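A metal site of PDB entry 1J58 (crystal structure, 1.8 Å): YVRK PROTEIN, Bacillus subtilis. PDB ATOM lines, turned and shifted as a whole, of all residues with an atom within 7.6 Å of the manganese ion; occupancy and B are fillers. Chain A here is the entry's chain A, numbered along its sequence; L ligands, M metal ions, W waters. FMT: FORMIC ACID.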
ATOM      1  N   MET A  84       7.898   7.102 -26.946  1.00  0.00           N
ATOM      2  CA  MET A  84       8.470   8.204 -26.168  1.00  0.00           C
ATOM      3  C   MET A  84       8.074   9.566 -26.718  1.00  0.00           C
ATOM      4  O   MET A  84       7.996   9.758 -27.932  1.00  0.00           O
ATOM      5  CB  MET A  84       9.999   8.087 -26.132  1.00  0.00           C
ATOM      6  CG  MET A  84      10.694   9.132 -25.271  1.00  0.00           C
ATOM      7  SD  MET A  84      12.573   8.759 -24.980  1.00  0.00           S
ATOM      8  CE  MET A  84      12.375   7.392 -23.628  1.00  0.00           C
ATOM      9  N   ARG A  92      16.562  13.315 -23.503  1.00  0.00           N
ATOM     10  CA  ARG A  92      16.497  11.941 -23.015  1.00  0.00           C
ATOM     11  C   ARG A  92      17.970  11.739 -22.643  1.00  0.00           C
ATOM     12  O   ARG A  92      18.837  11.668 -23.524  1.00  0.00           O
ATOM     13  CB  ARG A  92      16.097  10.962 -24.110  1.00  0.00           C
ATOM     14  CG  ARG A  92      16.295   9.499 -23.713  1.00  0.00           C
ATOM     15  CD  ARG A  92      15.450   9.091 -22.512  1.00  0.00           C
ATOM     16  NE  ARG A  92      15.680   7.678 -22.161  1.00  0.00           N
ATOM     17  CZ  ARG A  92      16.648   7.243 -21.360  1.00  0.00           C
ATOM     18  NH1 ARG A  92      17.487   8.108 -20.800  1.00  0.00           N
ATOM     19  NH2 ARG A  92      16.799   5.947 -21.141  1.00  0.00           N
ATOM     20  N   GLU A  93      18.242  11.670 -21.345  1.00  0.00           N
ATOM     21  CA  GLU A  93      19.597  11.534 -20.820  1.00  0.00           C
ATOM     22  C   GLU A  93      20.544  10.558 -21.501  1.00  0.00           C
ATOM     23  O   GLU A  93      20.165   9.442 -21.832  1.00  0.00           O
ATOM     24  CB  GLU A  93      19.542  11.190 -19.337  1.00  0.00           C
ATOM     25  CG  GLU A  93      20.913  11.224 -18.675  1.00  0.00           C
ATOM     26  CD  GLU A  93      20.907  10.773 -17.231  1.00  0.00           C
ATOM     27  OE1 GLU A  93      19.818  10.719 -16.606  1.00  0.00           O
ATOM     28  OE2 GLU A  93      21.999  10.498 -16.700  1.00  0.00           O
ATOM     29  N   HIS A  95      22.766   7.751 -22.344  1.00  0.00           N
ATOM     30  CA  HIS A  95      22.668   6.400 -21.804  1.00  0.00           C
ATOM     31  C   HIS A  95      23.055   5.348 -22.834  1.00  0.00           C
ATOM     32  O   HIS A  95      23.360   5.662 -23.979  1.00  0.00           O
ATOM     33  CB  HIS A  95      21.219   6.134 -21.387  1.00  0.00           C
ATOM     34  CG  HIS A  95      20.270   6.081 -22.542  1.00  0.00           C
ATOM     35  ND1 HIS A  95      19.751   7.213 -23.146  1.00  0.00           N
ATOM     36  CD2 HIS A  95      19.787   5.034 -23.248  1.00  0.00           C
ATOM     37  CE1 HIS A  95      19.008   6.865 -24.174  1.00  0.00           C
ATOM     38  NE2 HIS A  95      19.005   5.546 -24.261  1.00  0.00           N
ATOM     39  N   TRP A  96      23.023   4.091 -22.413  1.00  0.00           N
ATOM     40  CA  TRP A  96      23.309   2.974 -23.295  1.00  0.00           C
ATOM     41  C   TRP A  96      22.564   1.759 -22.749  1.00  0.00           C
ATOM     42  O   TRP A  96      22.056   1.795 -21.641  1.00  0.00           O
ATOM     43  CB  TRP A  96      24.824   2.709 -23.372  1.00  0.00           C
ATOM     44  CG  TRP A  96      25.453   2.030 -22.175  1.00  0.00           C
ATOM     45  CD1 TRP A  96      25.649   0.680 -22.000  1.00  0.00           C
ATOM     46  CD2 TRP A  96      25.987   2.655 -21.001  1.00  0.00           C
ATOM     47  NE1 TRP A  96      26.280   0.443 -20.801  1.00  0.00           N
ATOM     48  CE2 TRP A  96      26.492   1.630 -20.167  1.00  0.00           C
ATOM     49  CE3 TRP A  96      26.085   3.990 -20.572  1.00  0.00           C
ATOM     50  CZ2 TRP A  96      27.096   1.903 -18.932  1.00  0.00           C
ATOM     51  CZ3 TRP A  96      26.679   4.254 -19.336  1.00  0.00           C
ATOM     52  CH2 TRP A  96      27.180   3.216 -18.535  1.00  0.00           C
ATOM     53  N   HIS A  97      22.462   0.714 -23.555  1.00  0.00           N
ATOM     54  CA  HIS A  97      21.819  -0.507 -23.098  1.00  0.00           C
ATOM     55  C   HIS A  97      22.372  -1.704 -23.834  1.00  0.00           C
ATOM     56  O   HIS A  97      23.117  -1.558 -24.806  1.00  0.00           O
ATOM     57  CB  HIS A  97      20.285  -0.458 -23.256  1.00  0.00           C
ATOM     58  CG  HIS A  97      19.799   0.562 -24.234  1.00  0.00           C
ATOM     59  ND1 HIS A  97      20.074   0.498 -25.578  1.00  0.00           N
ATOM     60  CD2 HIS A  97      19.041   1.674 -24.046  1.00  0.00           C
ATOM     61  CE1 HIS A  97      19.505   1.517 -26.189  1.00  0.00           C
ATOM     62  NE2 HIS A  97      18.876   2.254 -25.280  1.00  0.00           N
ATOM     63  N   GLU A  99      20.644  -3.900 -25.511  1.00  0.00           N
ATOM     64  CA  GLU A  99      19.932  -4.088 -26.770  1.00  0.00           C
ATOM     65  C   GLU A  99      20.227  -3.041 -27.835  1.00  0.00           C
ATOM     66  O   GLU A  99      20.609  -1.912 -27.521  1.00  0.00           O
ATOM     67  CB  GLU A  99      18.418  -4.093 -26.502  1.00  0.00           C
ATOM     68  CG  GLU A  99      17.962  -5.127 -25.476  1.00  0.00           C
ATOM     69  CD  GLU A  99      17.976  -4.618 -24.037  1.00  0.00           C
ATOM     70  OE1 GLU A  99      18.568  -3.548 -23.774  1.00  0.00           O
ATOM     71  OE2 GLU A  99      17.397  -5.294 -23.170  1.00  0.00           O
ATOM     72  N   ALA A 100      20.072  -3.427 -29.097  1.00  0.00           N
ATOM     73  CA  ALA A 100      20.254  -2.494 -30.199  1.00  0.00           C
ATOM     74  C   ALA A 100      18.921  -1.741 -30.210  1.00  0.00           C
ATOM     75  O   ALA A 100      17.898  -2.289 -29.820  1.00  0.00           O
ATOM     76  CB  ALA A 100      20.446  -3.242 -31.524  1.00  0.00           C
ATOM     77  N   GLU A 101      18.955  -0.490 -30.658  1.00  0.00           N
ATOM     78  CA  GLU A 101      17.745   0.329 -30.686  1.00  0.00           C
ATOM     79  C   GLU A 101      17.451   0.910 -32.070  1.00  0.00           C
ATOM     80  O   GLU A 101      18.334   1.461 -32.722  1.00  0.00           O
ATOM     81  CB  GLU A 101      17.888   1.470 -29.682  1.00  0.00           C
ATOM     82  CG  GLU A 101      16.922   2.631 -29.870  1.00  0.00           C
ATOM     83  CD  GLU A 101      17.173   3.727 -28.851  1.00  0.00           C
ATOM     84  OE1 GLU A 101      16.885   4.904 -29.151  1.00  0.00           O
ATOM     85  OE2 GLU A 101      17.646   3.391 -27.739  1.00  0.00           O
ATOM     86  N   TRP A 132      16.622   5.921 -37.003  1.00  0.00           N
ATOM     87  CA  TRP A 132      17.962   5.868 -36.439  1.00  0.00           C
ATOM     88  C   TRP A 132      18.104   4.453 -35.917  1.00  0.00           C
ATOM     89  O   TRP A 132      17.108   3.757 -35.688  1.00  0.00           O
ATOM     90  CB  TRP A 132      18.213   6.926 -35.346  1.00  0.00           C
ATOM     91  CG  TRP A 132      17.544   6.770 -34.005  1.00  0.00           C
ATOM     92  CD1 TRP A 132      17.706   5.758 -33.102  1.00  0.00           C
ATOM     93  CD2 TRP A 132      16.687   7.739 -33.369  1.00  0.00           C
ATOM     94  NE1 TRP A 132      17.019   6.033 -31.947  1.00  0.00           N
ATOM     95  CE2 TRP A 132      16.384   7.245 -32.081  1.00  0.00           C
ATOM     96  CE3 TRP A 132      16.155   8.971 -33.772  1.00  0.00           C
ATOM     97  CZ2 TRP A 132      15.568   7.945 -31.187  1.00  0.00           C
ATOM     98  CZ3 TRP A 132      15.346   9.664 -32.876  1.00  0.00           C
ATOM     99  CH2 TRP A 132      15.064   9.157 -31.606  1.00  0.00           C
ATOM    100  N   PHE A 134      20.863   2.409 -33.252  1.00  0.00           N
ATOM    101  CA  PHE A 134      22.033   2.480 -32.389  1.00  0.00           C
ATOM    102  C   PHE A 134      22.427   1.068 -32.017  1.00  0.00           C
ATOM    103  O   PHE A 134      21.673   0.361 -31.347  1.00  0.00           O
ATOM    104  CB  PHE A 134      21.676   3.261 -31.123  1.00  0.00           C
ATOM    105  CG  PHE A 134      21.252   4.676 -31.374  1.00  0.00           C
ATOM    106  CD1 PHE A 134      20.366   5.311 -30.504  1.00  0.00           C
ATOM    107  CD2 PHE A 134      21.725   5.387 -32.464  1.00  0.00           C
ATOM    108  CE1 PHE A 134      19.971   6.621 -30.716  1.00  0.00           C
ATOM    109  CE2 PHE A 134      21.335   6.711 -32.693  1.00  0.00           C
ATOM    110  CZ  PHE A 134      20.452   7.326 -31.804  1.00  0.00           C
ATOM    111  N   LEU A 138      26.337   1.034 -27.607  1.00  0.00           N
ATOM    112  CA  LEU A 138      26.889   2.342 -27.936  1.00  0.00           C
ATOM    113  C   LEU A 138      26.051   3.427 -27.274  1.00  0.00           C
ATOM    114  O   LEU A 138      24.823   3.438 -27.396  1.00  0.00           O
ATOM    115  CB  LEU A 138      26.943   2.527 -29.463  1.00  0.00           C
ATOM    116  CG  LEU A 138      27.823   1.465 -30.149  1.00  0.00           C
ATOM    117  CD1 LEU A 138      27.991   1.798 -31.624  1.00  0.00           C
ATOM    118  CD2 LEU A 138      29.198   1.410 -29.459  1.00  0.00           C
ATOM    119  N   PRO A 139      26.707   4.362 -26.564  1.00  0.00           N
ATOM    120  CA  PRO A 139      26.032   5.454 -25.853  1.00  0.00           C
ATOM    121  C   PRO A 139      25.413   6.499 -26.770  1.00  0.00           C
ATOM    122  O   PRO A 139      26.008   6.890 -27.775  1.00  0.00           O
ATOM    123  CB  PRO A 139      27.148   6.016 -24.980  1.00  0.00           C
ATOM    124  CG  PRO A 139      28.345   5.873 -25.875  1.00  0.00           C
ATOM    125  CD  PRO A 139      28.169   4.485 -26.469  1.00  0.00           C
ATOM    126  N   HIS A 140      24.225   6.964 -26.397  1.00  0.00           N
ATOM    127  CA  HIS A 140      23.511   7.942 -27.201  1.00  0.00           C
ATOM    128  C   HIS A 140      22.580   8.829 -26.368  1.00  0.00           C
ATOM    129  O   HIS A 140      22.395   8.625 -25.169  1.00  0.00           O
ATOM    130  CB  HIS A 140      22.694   7.225 -28.272  1.00  0.00           C
ATOM    131  CG  HIS A 140      21.856   6.102 -27.737  1.00  0.00           C
ATOM    132  ND1 HIS A 140      22.360   4.834 -27.522  1.00  0.00           N
ATOM    133  CD2 HIS A 140      20.560   6.062 -27.349  1.00  0.00           C
ATOM    134  CE1 HIS A 140      21.402   4.056 -27.034  1.00  0.00           C
ATOM    135  NE2 HIS A 140      20.302   4.781 -26.912  1.00  0.00           N
ATOM    136  N   SER A 141      21.998   9.819 -27.038  1.00  0.00           N
ATOM    137  CA  SER A 141      21.070  10.756 -26.413  1.00  0.00           C
ATOM    138  C   SER A 141      20.102  11.265 -27.477  1.00  0.00           C
ATOM    139  O   SER A 141      20.348  11.125 -28.668  1.00  0.00           O
ATOM    140  CB  SER A 141      21.828  11.942 -25.820  1.00  0.00           C
ATOM    141  OG  SER A 141      22.453  12.693 -26.854  1.00  0.00           O
ATOM    142  N   ILE A 142      19.008  11.854 -27.013  1.00  0.00           N
ATOM    143  CA  ILE A 142      17.989  12.418 -27.896  1.00  0.00           C
ATOM    144  C   ILE A 142      17.565  13.744 -27.285  1.00  0.00           C
ATOM    145  O   ILE A 142      17.368  13.837 -26.081  1.00  0.00           O
ATOM    146  CB  ILE A 142      16.723  11.535 -27.970  1.00  0.00           C
ATOM    147  CG1 ILE A 142      17.092  10.077 -28.263  1.00  0.00           C
ATOM    148  CG2 ILE A 142      15.779  12.070 -29.032  1.00  0.00           C
ATOM    149  CD1 ILE A 142      15.941   9.107 -28.066  1.00  0.00           C
ATOM    150  N   LEU A 153      10.294   3.515 -30.463  1.00  0.00           N
ATOM    151  CA  LEU A 153      11.589   2.870 -30.341  1.00  0.00           C
ATOM    152  C   LEU A 153      11.338   1.366 -30.317  1.00  0.00           C
ATOM    153  O   LEU A 153      10.338   0.915 -29.766  1.00  0.00           O
ATOM    154  CB  LEU A 153      12.274   3.277 -29.031  1.00  0.00           C
ATOM    155  CG  LEU A 153      12.551   4.760 -28.802  1.00  0.00           C
ATOM    156  CD1 LEU A 153      13.000   4.972 -27.364  1.00  0.00           C
ATOM    157  CD2 LEU A 153      13.617   5.240 -29.770  1.00  0.00           C
ATOM    158  N   PHE A 155      13.474  -2.290 -29.521  1.00  0.00           N
ATOM    159  CA  PHE A 155      14.700  -2.888 -29.013  1.00  0.00           C
ATOM    160  C   PHE A 155      14.706  -4.372 -29.360  1.00  0.00           C
ATOM    161  O   PHE A 155      13.666  -5.014 -29.304  1.00  0.00           O
ATOM    162  CB  PHE A 155      14.760  -2.694 -27.501  1.00  0.00           C
ATOM    163  CG  PHE A 155      14.732  -1.247 -27.096  1.00  0.00           C
ATOM    164  CD1 PHE A 155      15.899  -0.495 -27.069  1.00  0.00           C
ATOM    165  CD2 PHE A 155      13.527  -0.621 -26.768  1.00  0.00           C
ATOM    166  CE1 PHE A 155      15.871   0.857 -26.745  1.00  0.00           C
ATOM    167  CE2 PHE A 155      13.482   0.728 -26.443  1.00  0.00           C
ATOM    168  CZ  PHE A 155      14.661   1.474 -26.436  1.00  0.00           C
ATOM    169  N   PHE A 160      13.310  -6.421 -22.683  1.00  0.00           N
ATOM    170  CA  PHE A 160      13.750  -5.058 -22.434  1.00  0.00           C
ATOM    171  C   PHE A 160      13.018  -4.505 -21.213  1.00  0.00           C
ATOM    172  O   PHE A 160      11.788  -4.614 -21.119  1.00  0.00           O
ATOM    173  CB  PHE A 160      13.455  -4.183 -23.653  1.00  0.00           C
ATOM    174  CG  PHE A 160      13.864  -2.745 -23.495  1.00  0.00           C
ATOM    175  CD1 PHE A 160      15.202  -2.386 -23.626  1.00  0.00           C
ATOM    176  CD2 PHE A 160      12.922  -1.758 -23.230  1.00  0.00           C
ATOM    177  CE1 PHE A 160      15.588  -1.051 -23.489  1.00  0.00           C
ATOM    178  CE2 PHE A 160      13.299  -0.433 -23.091  1.00  0.00           C
ATOM    179  CZ  PHE A 160      14.636  -0.074 -23.222  1.00  0.00           C
ATOM    180  N   THR A 165      18.702  -0.405 -19.311  1.00  0.00           N
ATOM    181  CA  THR A 165      19.293   0.908 -19.560  1.00  0.00           C
ATOM    182  C   THR A 165      20.174   1.530 -18.486  1.00  0.00           C
ATOM    183  O   THR A 165      19.793   1.669 -17.322  1.00  0.00           O
ATOM    184  CB  THR A 165      18.184   1.921 -19.910  1.00  0.00           C
ATOM    185  OG1 THR A 165      17.366   1.371 -20.961  1.00  0.00           O
ATOM    186  CG2 THR A 165      18.784   3.223 -20.388  1.00  0.00           C
ATOM    187  N   GLN A 167      22.132   4.864 -17.287  1.00  0.00           N
ATOM    188  CA  GLN A 167      22.169   6.320 -17.425  1.00  0.00           C
ATOM    189  C   GLN A 167      23.496   6.892 -16.945  1.00  0.00           C
ATOM    190  O   GLN A 167      24.048   6.446 -15.942  1.00  0.00           O
ATOM    191  CB  GLN A 167      21.050   6.980 -16.601  1.00  0.00           C
ATOM    192  CG  GLN A 167      19.822   7.395 -17.394  1.00  0.00           C
ATOM    193  CD  GLN A 167      18.991   6.218 -17.840  1.00  0.00           C
ATOM    194  OE1 GLN A 167      18.455   5.472 -17.013  1.00  0.00           O
ATOM    195  NE2 GLN A 167      18.881   6.042 -19.147  1.00  0.00           N
HETATM  196  C   FMT L   1      15.406   5.213 -24.613  1.00  0.00           C
HETATM  197  O1  FMT L   1      16.168   4.185 -25.044  1.00  0.00           O
HETATM  198  O2  FMT L   1      14.781   5.211 -23.574  1.00  0.00           O
HETATM  199 MN    MN M   1      18.261   4.370 -26.010  1.00  0.00          MN
HETATM  200  O   HOH W   1      17.385   6.219 -26.930  1.00  0.00           O
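The manganese ion is bound by OE2 of Glu 101.
The manganese ion is bound by a ring nitrogen (NE2) of His 95.
Water W1 binds the manganese ion (2.2 Å).
NE2 of His 140 is bound to the manganese ion, at 2.3 Å.
An oxygen (O1) of the ligand is bound to the manganese ion (2.3 Å).
NE2 of His 97 binds the manganese ion, at 2.3 Å.
The manganese ion has six donor atoms within binding distance.
The backbone NH (N) of Phe 134 sits at hydrogen-bond distance from the backbone carbonyl oxygen (O) of Glu 101 (2.8 Å).
The indole nitrogen (NE1) of Trp 132 is in hydrogen-bond range of the side-chain carboxylate (OE1) of Glu 101 (3.0 Å).
A ring nitrogen (ND1) of His 95 is in hydrogen-bond range of the guanidinium group (NH1) of Arg 92 (3.4 Å).
A ring nitrogen (ND1) of His 95 lies within hydrogen-bond range of the backbone carbonyl oxygen (O) of Glu 93.
A ring nitrogen (ND1) of His 140 sits at hydrogen-bond distance from the backbone carbonyl oxygen (O) of Leu 138, 2.8 Å away.
A ring nitrogen (ND1) of His 97 lies within hydrogen-bond range of the backbone carbonyl oxygen of Glu 99 (3.1 Å).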
